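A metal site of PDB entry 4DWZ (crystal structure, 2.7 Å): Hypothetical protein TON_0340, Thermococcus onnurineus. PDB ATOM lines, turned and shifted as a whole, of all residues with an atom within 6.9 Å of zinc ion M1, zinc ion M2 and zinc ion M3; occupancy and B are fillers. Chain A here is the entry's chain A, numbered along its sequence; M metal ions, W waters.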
ATOM      1  N   PHE A  50     -30.238  29.499   9.327  1.00  0.00           N
ATOM      2  CA  PHE A  50     -29.831  28.110   9.103  1.00  0.00           C
ATOM      3  C   PHE A  50     -30.987  27.182   9.492  1.00  0.00           C
ATOM      4  O   PHE A  50     -31.250  26.958  10.666  1.00  0.00           O
ATOM      5  CB  PHE A  50     -28.592  27.803   9.952  1.00  0.00           C
ATOM      6  CG  PHE A  50     -27.779  26.653   9.448  1.00  0.00           C
ATOM      7  CD1 PHE A  50     -26.584  26.878   8.782  1.00  0.00           C
ATOM      8  CD2 PHE A  50     -28.235  25.349   9.617  1.00  0.00           C
ATOM      9  CE1 PHE A  50     -25.846  25.811   8.287  1.00  0.00           C
ATOM     10  CE2 PHE A  50     -27.503  24.274   9.120  1.00  0.00           C
ATOM     11  CZ  PHE A  50     -26.309  24.512   8.457  1.00  0.00           C
ATOM     12  N   ILE A  52     -33.121  23.962  10.460  1.00  0.00           N
ATOM     13  CA  ILE A  52     -32.743  22.773  11.226  1.00  0.00           C
ATOM     14  C   ILE A  52     -33.688  21.600  11.026  1.00  0.00           C
ATOM     15  O   ILE A  52     -34.872  21.671  11.349  1.00  0.00           O
ATOM     16  CB  ILE A  52     -32.660  23.117  12.727  1.00  0.00           C
ATOM     17  CG1 ILE A  52     -31.489  24.066  12.947  1.00  0.00           C
ATOM     18  CG2 ILE A  52     -32.450  21.853  13.569  1.00  0.00           C
ATOM     19  CD1 ILE A  52     -31.370  24.553  14.323  1.00  0.00           C
ATOM     20  N   GLU A  59     -32.550  28.543  12.974  1.00  0.00           N
ATOM     21  CA  GLU A  59     -31.876  28.432  14.239  1.00  0.00           C
ATOM     22  C   GLU A  59     -31.635  29.786  14.916  1.00  0.00           C
ATOM     23  O   GLU A  59     -31.719  30.835  14.280  1.00  0.00           O
ATOM     24  CB  GLU A  59     -30.539  27.733  13.996  1.00  0.00           C
ATOM     25  CG  GLU A  59     -29.762  27.446  15.227  1.00  0.00           C
ATOM     26  CD  GLU A  59     -28.327  27.156  14.895  1.00  0.00           C
ATOM     27  OE1 GLU A  59     -28.080  26.535  13.828  1.00  0.00           O
ATOM     28  OE2 GLU A  59     -27.451  27.539  15.703  1.00  0.00           O
ATOM     29  N   THR A  60     -31.281  29.714  16.189  1.00  0.00           N
ATOM     30  CA  THR A  60     -31.013  30.859  17.049  1.00  0.00           C
ATOM     31  C   THR A  60     -29.609  31.468  16.851  1.00  0.00           C
ATOM     32  O   THR A  60     -29.375  32.633  17.185  1.00  0.00           O
ATOM     33  CB  THR A  60     -31.185  30.417  18.528  1.00  0.00           C
ATOM     34  OG1 THR A  60     -31.560  31.537  19.323  1.00  0.00           O
ATOM     35  CG2 THR A  60     -29.892  29.807  19.078  1.00  0.00           C
ATOM     36  N   ASP A  61     -28.668  30.688  16.310  1.00  0.00           N
ATOM     37  CA  ASP A  61     -27.319  31.202  16.052  1.00  0.00           C
ATOM     38  C   ASP A  61     -27.252  31.761  14.631  1.00  0.00           C
ATOM     39  O   ASP A  61     -27.621  31.080  13.668  1.00  0.00           O
ATOM     40  CB  ASP A  61     -26.281  30.079  16.199  1.00  0.00           C
ATOM     41  CG  ASP A  61     -24.871  30.556  15.944  1.00  0.00           C
ATOM     42  OD1 ASP A  61     -23.985  29.709  15.672  1.00  0.00           O
ATOM     43  OD2 ASP A  61     -24.631  31.786  16.015  1.00  0.00           O
ATOM     44  N   GLY A  62     -26.797  32.990  14.494  1.00  0.00           N
ATOM     45  CA  GLY A  62     -26.735  33.587  13.177  1.00  0.00           C
ATOM     46  C   GLY A  62     -27.371  34.960  13.148  1.00  0.00           C
ATOM     47  O   GLY A  62     -26.674  35.951  12.954  1.00  0.00           O
ATOM     48  N   GLU A 115     -23.567  32.179   9.625  1.00  0.00           N
ATOM     49  CA  GLU A 115     -24.284  30.931   9.850  1.00  0.00           C
ATOM     50  C   GLU A 115     -25.434  30.673   8.868  1.00  0.00           C
ATOM     51  O   GLU A 115     -26.606  30.735   9.231  1.00  0.00           O
ATOM     52  CB  GLU A 115     -24.822  30.919  11.289  1.00  0.00           C
ATOM     53  CG  GLU A 115     -25.380  29.585  11.726  1.00  0.00           C
ATOM     54  CD  GLU A 115     -24.308  28.543  11.948  1.00  0.00           C
ATOM     55  OE1 GLU A 115     -23.119  28.812  11.657  1.00  0.00           O
ATOM     56  OE2 GLU A 115     -24.652  27.431  12.393  1.00  0.00           O
ATOM     57  N   THR A 116     -25.071  30.369   7.625  1.00  0.00           N
ATOM     58  CA  THR A 116     -26.025  30.091   6.552  1.00  0.00           C
ATOM     59  C   THR A 116     -25.587  28.790   5.886  1.00  0.00           C
ATOM     60  O   THR A 116     -24.413  28.640   5.550  1.00  0.00           O
ATOM     61  CB  THR A 116     -26.005  31.204   5.491  1.00  0.00           C
ATOM     62  OG1 THR A 116     -26.222  32.470   6.135  1.00  0.00           O
ATOM     63  CG2 THR A 116     -27.093  30.991   4.461  1.00  0.00           C
ATOM     64  N   MET A 128     -25.501  19.493  10.938  1.00  0.00           N
ATOM     65  CA  MET A 128     -24.336  18.926  11.588  1.00  0.00           C
ATOM     66  C   MET A 128     -24.517  17.426  11.859  1.00  0.00           C
ATOM     67  O   MET A 128     -23.541  16.680  11.921  1.00  0.00           O
ATOM     68  CB  MET A 128     -24.031  19.682  12.891  1.00  0.00           C
ATOM     69  CG  MET A 128     -23.344  21.039  12.685  1.00  0.00           C
ATOM     70  SD  MET A 128     -21.842  21.001  11.625  1.00  0.00           S
ATOM     71  CE  MET A 128     -20.624  20.156  12.698  1.00  0.00           C
ATOM     72  N   VAL A 155     -18.866  33.537   7.997  1.00  0.00           N
ATOM     73  CA  VAL A 155     -18.574  33.201   9.391  1.00  0.00           C
ATOM     74  C   VAL A 155     -19.239  31.885   9.703  1.00  0.00           C
ATOM     75  O   VAL A 155     -20.441  31.746   9.479  1.00  0.00           O
ATOM     76  CB  VAL A 155     -19.103  34.239  10.374  1.00  0.00           C
ATOM     77  CG1 VAL A 155     -18.732  33.836  11.784  1.00  0.00           C
ATOM     78  CG2 VAL A 155     -18.553  35.618  10.064  1.00  0.00           C
ATOM     79  N   GLY A 156     -18.488  30.932  10.239  1.00  0.00           N
ATOM     80  CA  GLY A 156     -19.071  29.643  10.552  1.00  0.00           C
ATOM     81  C   GLY A 156     -18.381  28.964  11.711  1.00  0.00           C
ATOM     82  O   GLY A 156     -17.291  29.369  12.118  1.00  0.00           O
ATOM     83  N   ASP A 157     -19.004  27.912  12.244  1.00  0.00           N
ATOM     84  CA  ASP A 157     -18.470  27.181  13.372  1.00  0.00           C
ATOM     85  C   ASP A 157     -18.614  25.653  13.304  1.00  0.00           C
ATOM     86  O   ASP A 157     -18.398  24.978  14.299  1.00  0.00           O
ATOM     87  CB  ASP A 157     -19.112  27.691  14.661  1.00  0.00           C
ATOM     88  CG  ASP A 157     -20.621  27.601  14.635  1.00  0.00           C
ATOM     89  OD1 ASP A 157     -21.187  26.987  13.702  1.00  0.00           O
ATOM     90  OD2 ASP A 157     -21.262  28.143  15.559  1.00  0.00           O
ATOM     91  N   GLY A 158     -18.978  25.107  12.150  1.00  0.00           N
ATOM     92  CA  GLY A 158     -19.130  23.663  12.043  1.00  0.00           C
ATOM     93  C   GLY A 158     -18.632  22.989  10.765  1.00  0.00           C
ATOM     94  O   GLY A 158     -18.573  21.772  10.699  1.00  0.00           O
ATOM     95  N   GLY A 159     -18.303  23.782   9.742  1.00  0.00           N
ATOM     96  CA  GLY A 159     -17.805  23.201   8.501  1.00  0.00           C
ATOM     97  C   GLY A 159     -18.814  22.996   7.373  1.00  0.00           C
ATOM     98  O   GLY A 159     -18.427  22.642   6.273  1.00  0.00           O
ATOM     99  N   ASN A 160     -20.092  23.228   7.623  1.00  0.00           N
ATOM    100  CA  ASN A 160     -21.118  23.032   6.590  1.00  0.00           C
ATOM    101  C   ASN A 160     -21.814  24.340   6.250  1.00  0.00           C
ATOM    102  O   ASN A 160     -22.925  24.341   5.726  1.00  0.00           O
ATOM    103  CB  ASN A 160     -22.174  22.052   7.063  1.00  0.00           C
ATOM    104  CG  ASN A 160     -23.032  22.611   8.190  1.00  0.00           C
ATOM    105  OD1 ASN A 160     -22.663  23.600   8.834  1.00  0.00           O
ATOM    106  ND2 ASN A 160     -24.164  21.968   8.442  1.00  0.00           N
ATOM    107  N   GLU A 161     -21.141  25.447   6.544  1.00  0.00           N
ATOM    108  CA  GLU A 161     -21.703  26.764   6.295  1.00  0.00           C
ATOM    109  C   GLU A 161     -21.081  27.407   5.056  1.00  0.00           C
ATOM    110  O   GLU A 161     -20.128  26.892   4.475  1.00  0.00           O
ATOM    111  CB  GLU A 161     -21.490  27.671   7.512  1.00  0.00           C
ATOM    112  CG  GLU A 161     -22.019  27.102   8.828  1.00  0.00           C
ATOM    113  CD  GLU A 161     -20.969  26.301   9.594  1.00  0.00           C
ATOM    114  OE1 GLU A 161     -20.140  25.611   8.959  1.00  0.00           O
ATOM    115  OE2 GLU A 161     -20.971  26.348  10.833  1.00  0.00           O
ATOM    116  N   ALA A 194     -16.354  29.140  17.766  1.00  0.00           N
ATOM    117  CA  ALA A 194     -17.007  28.085  18.515  1.00  0.00           C
ATOM    118  C   ALA A 194     -18.518  28.245  18.278  1.00  0.00           C
ATOM    119  O   ALA A 194     -19.235  27.258  18.171  1.00  0.00           O
ATOM    120  CB  ALA A 194     -16.666  28.228  19.971  1.00  0.00           C
ATOM    121  N   VAL A 195     -18.957  29.500  18.214  1.00  0.00           N
ATOM    122  CA  VAL A 195     -20.363  29.857  17.964  1.00  0.00           C
ATOM    123  C   VAL A 195     -20.279  30.998  16.945  1.00  0.00           C
ATOM    124  O   VAL A 195     -19.553  31.973  17.153  1.00  0.00           O
ATOM    125  CB  VAL A 195     -21.102  30.386  19.264  1.00  0.00           C
ATOM    126  CG1 VAL A 195     -22.568  30.643  18.942  1.00  0.00           C
ATOM    127  CG2 VAL A 195     -21.013  29.386  20.403  1.00  0.00           C
ATOM    128  N   SER A 196     -21.026  30.905  15.848  1.00  0.00           N
ATOM    129  CA  SER A 196     -20.940  31.930  14.818  1.00  0.00           C
ATOM    130  C   SER A 196     -21.274  33.362  15.223  1.00  0.00           C
ATOM    131  O   SER A 196     -20.665  34.291  14.697  1.00  0.00           O
ATOM    132  CB  SER A 196     -21.768  31.535  13.593  1.00  0.00           C
ATOM    133  OG  SER A 196     -21.238  30.358  13.007  1.00  0.00           O
ATOM    134  N   ASN A 197     -22.207  33.557  16.153  1.00  0.00           N
ATOM    135  CA  ASN A 197     -22.512  34.920  16.581  1.00  0.00           C
ATOM    136  C   ASN A 197     -21.247  35.573  17.180  1.00  0.00           C
ATOM    137  O   ASN A 197     -20.982  36.764  16.971  1.00  0.00           O
ATOM    138  CB  ASN A 197     -23.645  34.937  17.619  1.00  0.00           C
ATOM    139  CG  ASN A 197     -24.980  34.473  17.050  1.00  0.00           C
ATOM    140  OD1 ASN A 197     -25.399  34.894  15.955  1.00  0.00           O
ATOM    141  ND2 ASN A 197     -25.664  33.615  17.790  1.00  0.00           N
ATOM    142  N   ASP A 235     -33.370  26.598  19.192  1.00  0.00           N
ATOM    143  CA  ASP A 235     -31.991  26.358  19.599  1.00  0.00           C
ATOM    144  C   ASP A 235     -31.567  25.138  18.789  1.00  0.00           C
ATOM    145  O   ASP A 235     -32.191  24.077  18.894  1.00  0.00           O
ATOM    146  CB  ASP A 235     -31.890  26.060  21.099  1.00  0.00           C
ATOM    147  CG  ASP A 235     -30.467  25.788  21.540  1.00  0.00           C
ATOM    148  OD1 ASP A 235     -29.841  26.702  22.112  1.00  0.00           O
ATOM    149  OD2 ASP A 235     -29.971  24.655  21.319  1.00  0.00           O
ATOM    150  N   GLY A 236     -30.525  25.300  17.995  1.00  0.00           N
ATOM    151  CA  GLY A 236     -30.032  24.237  17.138  1.00  0.00           C
ATOM    152  C   GLY A 236     -29.784  22.872  17.745  1.00  0.00           C
ATOM    153  O   GLY A 236     -29.984  21.861  17.081  1.00  0.00           O
ATOM    154  N   VAL A 237     -29.339  22.826  18.998  1.00  0.00           N
ATOM    155  CA  VAL A 237     -29.047  21.552  19.621  1.00  0.00           C
ATOM    156  C   VAL A 237     -30.238  20.891  20.291  1.00  0.00           C
ATOM    157  O   VAL A 237     -30.534  19.730  20.018  1.00  0.00           O
ATOM    158  CB  VAL A 237     -27.915  21.691  20.653  1.00  0.00           C
ATOM    159  CG1 VAL A 237     -27.501  20.323  21.141  1.00  0.00           C
ATOM    160  CG2 VAL A 237     -26.717  22.389  20.014  1.00  0.00           C
ATOM    161  N   VAL A 245     -28.288  29.430  22.718  1.00  0.00           N
ATOM    162  CA  VAL A 245     -27.658  29.318  21.404  1.00  0.00           C
ATOM    163  C   VAL A 245     -26.711  28.132  21.353  1.00  0.00           C
ATOM    164  O   VAL A 245     -25.851  27.986  22.220  1.00  0.00           O
ATOM    165  CB  VAL A 245     -26.870  30.588  21.053  1.00  0.00           C
ATOM    166  CG1 VAL A 245     -26.369  30.496  19.625  1.00  0.00           C
ATOM    167  CG2 VAL A 245     -27.732  31.811  21.232  1.00  0.00           C
ATOM    168  N   ASP A 246     -26.856  27.311  20.318  1.00  0.00           N
ATOM    169  CA  ASP A 246     -26.040  26.113  20.133  1.00  0.00           C
ATOM    170  C   ASP A 246     -25.907  25.340  21.440  1.00  0.00           C
ATOM    171  O   ASP A 246     -24.795  24.962  21.828  1.00  0.00           O
ATOM    172  CB  ASP A 246     -24.666  26.481  19.607  1.00  0.00           C
ATOM    173  CG  ASP A 246     -24.703  27.014  18.196  1.00  0.00           C
ATOM    174  OD1 ASP A 246     -25.667  26.715  17.470  1.00  0.00           O
ATOM    175  OD2 ASP A 246     -23.761  27.721  17.798  1.00  0.00           O
ATOM    176  N   GLY A 247     -27.042  25.147  22.108  1.00  0.00           N
ATOM    177  CA  GLY A 247     -27.069  24.422  23.370  1.00  0.00           C
ATOM    178  C   GLY A 247     -26.369  25.062  24.554  1.00  0.00           C
ATOM    179  O   GLY A 247     -26.265  24.441  25.611  1.00  0.00           O
HETATM  180 ZN    ZN M   1     -23.648  27.542  15.603  1.00  0.00          ZN
HETATM  181 ZN    ZN M   2     -22.739  26.111  12.189  1.00  0.00          ZN
HETATM  182 ZN    ZN M   3     -26.548  25.721  15.775  1.00  0.00          ZN
HETATM  183  O   HOH W   1     -23.821  24.283  10.949  1.00  0.00           O
HETATM  184  O   HOH W   2     -25.391  26.646  14.554  1.00  0.00           O
HETATM  185  O   HOH W   3     -26.764  23.348  16.082  1.00  0.00           O
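The side-chain carboxylate (OE2) of Glu 59 lies close to the backbone NH (N) of Asp 61. O of Phe 50 is in hydrogen-bond range of N of Glu 59, 3.1 Å away. OD1 of Asp 61 sits close to N of Ser 196 (3.2 Å). OD2 of Asp 61 is in hydrogen-bond range of ND2 of Asn 197 (2.8 Å). The backbone NH (N) of Gly 158 sits at hydrogen-bond distance from the side-chain carboxylate (OE1) of Glu 161 (3.4 Å). The side-chain carboxylate of Glu 161 sits close to the side-chain amide oxygen of Asn 160 (3.2 Å). The backbone NH (N) of Gly 159 sits at hydrogen-bond distance from the side-chain carboxylate (OE1) of Glu 161 (2.7 Å). The side-chain carboxylate of Glu 115 is in hydrogen-bond range of the side-chain hydroxyl of Ser 196 (2.8 Å).
Five residues have an atom within 4 Å of zinc ion M1: Glu 59, Asp 61, Glu 115, Asp 157 and Asp 246.
Gly 158 touches zinc ion M2. Of the 26 residues printed, 4 come within 4 Å of zinc ion M2.
Two residues have an atom within 4 Å of zinc ion M3: Glu 59 and Asp 246. Along chain A the residues within 4 Å of zinc ion M3 span positions 59 to 246.
OD1 of Asp 61 binds zinc ion M1, 2.2 Å away. The side-chain carboxylate (OD2) of Asp 246 binds zinc ion M1, 2.2 Å away. Water W2 is bound to zinc ion M1, at 2.2 Å. Zinc ion M1 is bound by the side-chain carboxylate (OD2) of Asp 157 (2.5 Å). Zinc ion M1 has four donor atoms within binding distance.
Zinc ion M2 is bound by OE2 of Glu 161 (2.2 Å). The side-chain carboxylate (OE2) of Glu 115 binds zinc ion M2, 2.3 Å away. The side-chain carboxylate (OD1) of Asp 157 is bound to zinc ion M2 (2.3 Å). Water W1 binds zinc ion M2, at 2.5 Å. Zinc ion M2 has four donor atoms within binding distance. Slightly farther from zinc ion M2 lies the side-chain carboxylate (OE1) of Glu 115 (2.8 Å).
Zinc ion M3 is bound by water W2. OE2 of Glu 59 binds zinc ion M3 (2.0 Å). OD1 of Asp 246 is bound to zinc ion M3 (2.2 Å). Zinc ion M3 is bound by water W3 (2.4 Å). Zinc ion M3 has four donor atoms within binding distance. Slightly farther from zinc ion M3 lies the side-chain carboxylate (OE1) of Glu 59 (2.6 Å).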
